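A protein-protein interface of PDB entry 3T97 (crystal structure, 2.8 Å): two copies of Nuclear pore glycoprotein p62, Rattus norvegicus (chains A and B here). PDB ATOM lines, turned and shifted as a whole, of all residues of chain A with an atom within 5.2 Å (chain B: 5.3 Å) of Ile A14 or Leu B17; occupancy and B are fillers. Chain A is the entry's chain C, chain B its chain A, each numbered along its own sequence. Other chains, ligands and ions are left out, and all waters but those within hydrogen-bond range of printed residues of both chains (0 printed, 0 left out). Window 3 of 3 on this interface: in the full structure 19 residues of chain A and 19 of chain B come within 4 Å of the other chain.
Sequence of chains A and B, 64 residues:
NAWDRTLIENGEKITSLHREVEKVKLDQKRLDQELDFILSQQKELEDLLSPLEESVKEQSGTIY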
ATOM      1  N   GLU A   9     -20.290  18.613  -7.797  1.00  0.00           N
ATOM      2  CA  GLU A   9     -19.350  18.578  -6.685  1.00  0.00           C
ATOM      3  C   GLU A   9     -18.026  17.938  -7.096  1.00  0.00           C
ATOM      4  O   GLU A   9     -16.948  18.443  -6.771  1.00  0.00           O
ATOM      5  CB  GLU A   9     -19.964  17.796  -5.530  1.00  0.00           C
ATOM      6  CG  GLU A   9     -21.368  18.258  -5.200  1.00  0.00           C
ATOM      7  CD  GLU A   9     -21.834  17.793  -3.843  1.00  0.00           C
ATOM      8  OE1 GLU A   9     -22.387  16.672  -3.737  1.00  0.00           O
ATOM      9  OE2 GLU A   9     -21.631  18.557  -2.877  1.00  0.00           O
ATOM     10  N   ASN A  10     -18.120  16.818  -7.807  1.00  0.00           N
ATOM     11  CA  ASN A  10     -16.956  16.096  -8.302  1.00  0.00           C
ATOM     12  C   ASN A  10     -16.198  17.003  -9.257  1.00  0.00           C
ATOM     13  O   ASN A  10     -14.992  17.160  -9.141  1.00  0.00           O
ATOM     14  CB  ASN A  10     -17.385  14.828  -9.042  1.00  0.00           C
ATOM     15  CG  ASN A  10     -18.082  13.822  -8.138  1.00  0.00           C
ATOM     16  OD1 ASN A  10     -17.880  13.818  -6.921  1.00  0.00           O
ATOM     17  ND2 ASN A  10     -18.891  12.949  -8.735  1.00  0.00           N
ATOM     18  N   GLY A  11     -16.917  17.592 -10.206  1.00  0.00           N
ATOM     19  CA  GLY A  11     -16.304  18.498 -11.151  1.00  0.00           C
ATOM     20  C   GLY A  11     -15.627  19.648 -10.426  1.00  0.00           C
ATOM     21  O   GLY A  11     -14.613  20.162 -10.895  1.00  0.00           O
ATOM     22  N   GLU A  12     -16.194  20.058  -9.292  1.00  0.00           N
ATOM     23  CA  GLU A  12     -15.633  21.129  -8.471  1.00  0.00           C
ATOM     24  C   GLU A  12     -14.388  20.631  -7.733  1.00  0.00           C
ATOM     25  O   GLU A  12     -13.332  21.251  -7.777  1.00  0.00           O
ATOM     26  CB  GLU A  12     -16.652  21.643  -7.435  1.00  0.00           C
ATOM     27  CG  GLU A  12     -17.930  22.289  -8.004  1.00  0.00           C
ATOM     28  CD  GLU A  12     -18.753  23.057  -6.947  1.00  0.00           C
ATOM     29  OE1 GLU A  12     -18.882  22.566  -5.803  1.00  0.00           O
ATOM     30  OE2 GLU A  12     -19.281  24.147  -7.265  1.00  0.00           O
ATOM     31  N   LYS A  13     -14.520  19.507  -7.044  1.00  0.00           N
ATOM     32  CA  LYS A  13     -13.383  18.942  -6.324  1.00  0.00           C
ATOM     33  C   LYS A  13     -12.206  18.748  -7.273  1.00  0.00           C
ATOM     34  O   LYS A  13     -11.075  19.056  -6.924  1.00  0.00           O
ATOM     35  CB  LYS A  13     -13.756  17.600  -5.669  1.00  0.00           C
ATOM     36  CG  LYS A  13     -14.511  17.728  -4.357  1.00  0.00           C
ATOM     37  CD  LYS A  13     -15.012  16.380  -3.830  1.00  0.00           C
ATOM     38  CE  LYS A  13     -13.958  15.642  -3.013  1.00  0.00           C
ATOM     39  NZ  LYS A  13     -14.527  14.426  -2.350  1.00  0.00           N
ATOM     40  N   ILE A  14     -12.472  18.239  -8.471  1.00  0.00           N
ATOM     41  CA  ILE A  14     -11.416  18.012  -9.459  1.00  0.00           C
ATOM     42  C   ILE A  14     -10.514  19.248  -9.599  1.00  0.00           C
ATOM     43  O   ILE A  14      -9.302  19.176  -9.429  1.00  0.00           O
ATOM     44  CB  ILE A  14     -12.008  17.679 -10.850  1.00  0.00           C
ATOM     45  CG1 ILE A  14     -12.879  16.425 -10.769  1.00  0.00           C
ATOM     46  CG2 ILE A  14     -10.893  17.431 -11.850  1.00  0.00           C
ATOM     47  CD1 ILE A  14     -12.116  15.172 -10.405  1.00  0.00           C
ATOM     48  N   THR A  15     -11.126  20.383  -9.906  1.00  0.00           N
ATOM     49  CA  THR A  15     -10.393  21.624 -10.082  1.00  0.00           C
ATOM     50  C   THR A  15      -9.692  22.069  -8.813  1.00  0.00           C
ATOM     51  O   THR A  15      -8.574  22.561  -8.866  1.00  0.00           O
ATOM     52  CB  THR A  15     -11.331  22.734 -10.526  1.00  0.00           C
ATOM     53  OG1 THR A  15     -12.484  22.739  -9.674  1.00  0.00           O
ATOM     54  CG2 THR A  15     -11.763  22.530 -11.962  1.00  0.00           C
ATOM     55  N   SER A  16     -10.355  21.914  -7.673  1.00  0.00           N
ATOM     56  CA  SER A  16      -9.759  22.297  -6.397  1.00  0.00           C
ATOM     57  C   SER A  16      -8.523  21.455  -6.188  1.00  0.00           C
ATOM     58  O   SER A  16      -7.421  21.973  -6.048  1.00  0.00           O
ATOM     59  CB  SER A  16     -10.719  22.048  -5.231  1.00  0.00           C
ATOM     60  OG  SER A  16     -11.981  22.648  -5.443  1.00  0.00           O
ATOM     61  N   LEU A  17      -8.717  20.143  -6.173  1.00  0.00           N
ATOM     62  CA  LEU A  17      -7.623  19.213  -5.963  1.00  0.00           C
ATOM     63  C   LEU A  17      -6.522  19.482  -6.974  1.00  0.00           C
ATOM     64  O   LEU A  17      -5.346  19.241  -6.710  1.00  0.00           O
ATOM     65  CB  LEU A  17      -8.123  17.762  -6.068  1.00  0.00           C
ATOM     66  CG  LEU A  17      -9.211  17.294  -5.077  1.00  0.00           C
ATOM     67  CD1 LEU A  17      -9.494  15.830  -5.308  1.00  0.00           C
ATOM     68  CD2 LEU A  17      -8.776  17.516  -3.643  1.00  0.00           C
ATOM     69  N   HIS A  18      -6.908  20.009  -8.127  1.00  0.00           N
ATOM     70  CA  HIS A  18      -5.938  20.308  -9.167  1.00  0.00           C
ATOM     71  C   HIS A  18      -4.910  21.334  -8.703  1.00  0.00           C
ATOM     72  O   HIS A  18      -3.713  21.125  -8.868  1.00  0.00           O
ATOM     73  CB  HIS A  18      -6.648  20.829 -10.405  1.00  0.00           C
ATOM     74  CG  HIS A  18      -5.820  20.751 -11.645  1.00  0.00           C
ATOM     75  ND1 HIS A  18      -5.728  19.606 -12.402  1.00  0.00           N
ATOM     76  CD2 HIS A  18      -5.011  21.662 -12.235  1.00  0.00           C
ATOM     77  CE1 HIS A  18      -4.896  19.813 -13.405  1.00  0.00           C
ATOM     78  NE2 HIS A  18      -4.447  21.052 -13.327  1.00  0.00           N
ATOM     79  N   VAL A  21      -2.491  20.067  -5.681  1.00  0.00           N
ATOM     80  CA  VAL A  21      -1.380  19.296  -6.198  1.00  0.00           C
ATOM     81  C   VAL A  21      -0.369  20.209  -6.868  1.00  0.00           C
ATOM     82  O   VAL A  21       0.820  20.090  -6.624  1.00  0.00           O
ATOM     83  CB  VAL A  21      -1.861  18.233  -7.217  1.00  0.00           C
ATOM     84  CG1 VAL A  21      -0.680  17.561  -7.872  1.00  0.00           C
ATOM     85  CG2 VAL A  21      -2.705  17.195  -6.517  1.00  0.00           C
ATOM     86  N   ASN B  10     -14.468  12.544 -16.213  1.00  0.00           N
ATOM     87  CA  ASN B  10     -14.064  12.732 -14.823  1.00  0.00           C
ATOM     88  C   ASN B  10     -13.234  11.549 -14.341  1.00  0.00           C
ATOM     89  O   ASN B  10     -12.286  11.731 -13.582  1.00  0.00           O
ATOM     90  CB  ASN B  10     -15.280  12.882 -13.915  1.00  0.00           C
ATOM     91  CG  ASN B  10     -15.959  14.201 -14.084  1.00  0.00           C
ATOM     92  OD1 ASN B  10     -15.368  15.153 -14.585  1.00  0.00           O
ATOM     93  ND2 ASN B  10     -17.204  14.280 -13.647  1.00  0.00           N
ATOM     94  N   LYS B  13      -9.942  12.278 -15.466  1.00  0.00           N
ATOM     95  CA  LYS B  13      -9.411  13.405 -14.712  1.00  0.00           C
ATOM     96  C   LYS B  13      -8.957  12.970 -13.315  1.00  0.00           C
ATOM     97  O   LYS B  13      -7.932  13.427 -12.802  1.00  0.00           O
ATOM     98  CB  LYS B  13     -10.464  14.521 -14.607  1.00  0.00           C
ATOM     99  CG  LYS B  13     -10.226  15.672 -15.580  1.00  0.00           C
ATOM    100  CD  LYS B  13     -11.239  16.805 -15.437  1.00  0.00           C
ATOM    101  CE  LYS B  13     -12.595  16.450 -16.057  1.00  0.00           C
ATOM    102  NZ  LYS B  13     -13.533  17.620 -16.137  1.00  0.00           N
ATOM    103  N   ILE B  14      -9.731  12.077 -12.710  1.00  0.00           N
ATOM    104  CA  ILE B  14      -9.450  11.556 -11.379  1.00  0.00           C
ATOM    105  C   ILE B  14      -8.182  10.702 -11.394  1.00  0.00           C
ATOM    106  O   ILE B  14      -7.370  10.756 -10.467  1.00  0.00           O
ATOM    107  CB  ILE B  14     -10.673  10.744 -10.858  1.00  0.00           C
ATOM    108  CG1 ILE B  14     -11.828  11.706 -10.579  1.00  0.00           C
ATOM    109  CG2 ILE B  14     -10.337   9.988  -9.599  1.00  0.00           C
ATOM    110  CD1 ILE B  14     -13.166  11.037 -10.416  1.00  0.00           C
ATOM    111  N   THR B  15      -7.998   9.930 -12.456  1.00  0.00           N
ATOM    112  CA  THR B  15      -6.803   9.098 -12.566  1.00  0.00           C
ATOM    113  C   THR B  15      -5.552   9.959 -12.730  1.00  0.00           C
ATOM    114  O   THR B  15      -4.454   9.526 -12.387  1.00  0.00           O
ATOM    115  CB  THR B  15      -6.889   8.132 -13.759  1.00  0.00           C
ATOM    116  OG1 THR B  15      -8.107   7.384 -13.684  1.00  0.00           O
ATOM    117  CG2 THR B  15      -5.736   7.165 -13.739  1.00  0.00           C
ATOM    118  N   SER B  16      -5.717  11.169 -13.263  1.00  0.00           N
ATOM    119  CA  SER B  16      -4.596  12.093 -13.432  1.00  0.00           C
ATOM    120  C   SER B  16      -4.171  12.611 -12.064  1.00  0.00           C
ATOM    121  O   SER B  16      -2.986  12.591 -11.729  1.00  0.00           O
ATOM    122  CB  SER B  16      -4.975  13.279 -14.323  1.00  0.00           C
ATOM    123  OG  SER B  16      -5.034  12.901 -15.677  1.00  0.00           O
ATOM    124  N   LEU B  17      -5.148  13.088 -11.296  1.00  0.00           N
ATOM    125  CA  LEU B  17      -4.895  13.573  -9.949  1.00  0.00           C
ATOM    126  C   LEU B  17      -4.249  12.460  -9.143  1.00  0.00           C
ATOM    127  O   LEU B  17      -3.308  12.705  -8.368  1.00  0.00           O
ATOM    128  CB  LEU B  17      -6.194  13.971  -9.258  1.00  0.00           C
ATOM    129  CG  LEU B  17      -6.811  15.309  -9.612  1.00  0.00           C
ATOM    130  CD1 LEU B  17      -8.147  15.434  -8.926  1.00  0.00           C
ATOM    131  CD2 LEU B  17      -5.886  16.413  -9.166  1.00  0.00           C
ATOM    132  N   HIS B  18      -4.762  11.243  -9.323  1.00  0.00           N
ATOM    133  CA  HIS B  18      -4.240  10.089  -8.620  1.00  0.00           C
ATOM    134  C   HIS B  18      -2.760   9.829  -8.860  1.00  0.00           C
ATOM    135  O   HIS B  18      -2.040   9.428  -7.945  1.00  0.00           O
ATOM    136  CB  HIS B  18      -4.992   8.835  -9.008  1.00  0.00           C
ATOM    137  CG  HIS B  18      -4.478   7.606  -8.320  1.00  0.00           C
ATOM    138  ND1 HIS B  18      -4.783   7.305  -7.007  1.00  0.00           N
ATOM    139  CD2 HIS B  18      -3.603   6.654  -8.732  1.00  0.00           C
ATOM    140  CE1 HIS B  18      -4.115   6.224  -6.642  1.00  0.00           C
ATOM    141  NE2 HIS B  18      -3.392   5.811  -7.670  1.00  0.00           N
ATOM    142  N   ARG B  19      -2.309  10.039 -10.089  1.00  0.00           N
ATOM    143  CA  ARG B  19      -0.915   9.818 -10.433  1.00  0.00           C
ATOM    144  C   ARG B  19      -0.031  10.975 -10.041  1.00  0.00           C
ATOM    145  O   ARG B  19       1.124  10.790  -9.686  1.00  0.00           O
ATOM    146  CB  ARG B  19      -0.774   9.555 -11.922  1.00  0.00           C
ATOM    147  CG  ARG B  19      -1.396   8.243 -12.372  1.00  0.00           C
ATOM    148  CD  ARG B  19      -1.233   8.072 -13.867  1.00  0.00           C
ATOM    149  NE  ARG B  19      -2.112   7.031 -14.390  1.00  0.00           N
ATOM    150  CZ  ARG B  19      -1.817   5.741 -14.420  1.00  0.00           C
ATOM    151  NH1 ARG B  19      -2.692   4.880 -14.909  1.00  0.00           N
ATOM    152  NH2 ARG B  19      -0.640   5.316 -13.991  1.00  0.00           N
ATOM    153  N   GLU B  20      -0.570  12.178 -10.107  1.00  0.00           N
ATOM    154  CA  GLU B  20       0.206  13.342  -9.715  1.00  0.00           C
ATOM    155  C   GLU B  20       0.501  13.224  -8.229  1.00  0.00           C
ATOM    156  O   GLU B  20       1.592  13.553  -7.764  1.00  0.00           O
ATOM    157  CB  GLU B  20      -0.584  14.615 -10.004  1.00  0.00           C
ATOM    158  CG  GLU B  20      -0.939  14.771 -11.475  1.00  0.00           C
ATOM    159  CD  GLU B  20       0.274  15.078 -12.341  1.00  0.00           C
ATOM    160  OE1 GLU B  20       0.800  16.210 -12.240  1.00  0.00           O
ATOM    161  OE2 GLU B  20       0.695  14.185 -13.110  1.00  0.00           O
ATOM    162  N   VAL B  21      -0.481  12.738  -7.485  1.00  0.00           N
ATOM    163  CA  VAL B  21      -0.333  12.561  -6.054  1.00  0.00           C
ATOM    164  C   VAL B  21       0.666  11.444  -5.738  1.00  0.00           C
ATOM    165  O   VAL B  21       1.480  11.560  -4.829  1.00  0.00           O
ATOM    166  CB  VAL B  21      -1.701  12.266  -5.417  1.00  0.00           C
ATOM    167  CG1 VAL B  21      -1.529  11.646  -4.041  1.00  0.00           C
ATOM    168  CG2 VAL B  21      -2.488  13.551  -5.323  1.00  0.00           C
ATOM    169  N   GLU B  22       0.604  10.364  -6.502  1.00  0.00           N
ATOM    170  CA  GLU B  22       1.492   9.236  -6.286  1.00  0.00           C
ATOM    171  C   GLU B  22       2.928   9.654  -6.535  1.00  0.00           C
ATOM    172  O   GLU B  22       3.829   9.279  -5.799  1.00  0.00           O
ATOM    173  CB  GLU B  22       1.117   8.073  -7.213  1.00  0.00           C
ATOM    174  CG  GLU B  22      -0.276   7.518  -6.988  1.00  0.00           C
ATOM    175  CD  GLU B  22      -0.529   7.128  -5.535  1.00  0.00           C
ATOM    176  OE1 GLU B  22       0.347   6.434  -4.955  1.00  0.00           O
ATOM    177  OE2 GLU B  22      -1.595   7.505  -4.976  1.00  0.00           O
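Ile A14 touches Lys B13, but with the chains exchanged Lys A13 does not touch Ile B14 (7.8 Å).
Ile A14 touches its own counterpart, Ile B14.
Leu A17 touches its own counterpart, Leu B17.
Val B21 touches its own counterpart, Val A21.
Of the 7 pairs that touch across the chains among the printed residues, 3 have their exchanged pair printed and touching as well.
Ile A14 touches just these residues of chain B: Lys B13 (3.7 Å), Ile B14 (3.5 Å) and Leu B17 (3.9 Å).
Of chain A, only Ile A14 (3.9 Å), Leu A17 (3.7 Å) and His A18 (3.9 Å) come within 4 Å of Leu B17.
Of the printed residues of chain B, Val A21 touches Glu B20 (3.6 Å) and Val B21 (3.8 Å).
Of the printed residues of chain B, His A18 touches Leu B17 (3.9 Å).
Printed residues of chain A within 4 Å of Glu B20: Val A21.
Glu A12 touches none of the printed residues of chain B.
The nearest residue of chain B that does not touch Ile A14 is Asn B10 (4.7 Å).
The nearest residue of chain A that does not touch Leu B17 is Val A21 (4.2 Å).
The nearest printed residue of chain B that does not touch Leu A17 is Val B21 (6.5 Å).
Ile A14 touches Lys B13 (CG2 to CD, 3.7 Å).
CD1 of Ile A14 touches CG1 of Ile B14, at 3.5 Å.
Ile A14 touches Leu B17.
Leu A17 touches Leu B17 (CB to CD1, 3.7 Å).
CD2 of Leu B17 touches N of His A18 (3.9 Å).
CG1 of Val A21 touches CB of Glu B20 (3.6 Å).
CG2 of Val B21 touches CG2 of Val A21, at 3.8 Å.
Printed residues of chain A that touch a printed residue of chain B: Ile A14, Leu A17, His A18 and Val A21.
Hydrophobic or aromatic side chains of chain B that line the printed part of chain A: Ile B14, Leu B17 and Val B21.
Among the printed residues, no Asp or Glu carboxylate lies within 4 Å of a Lys or Arg side-chain nitrogen of the other chain.
The side-chain amide oxygen of Asn B10 lies close to the side-chain amino group of Lys B13 (3.4 Å).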
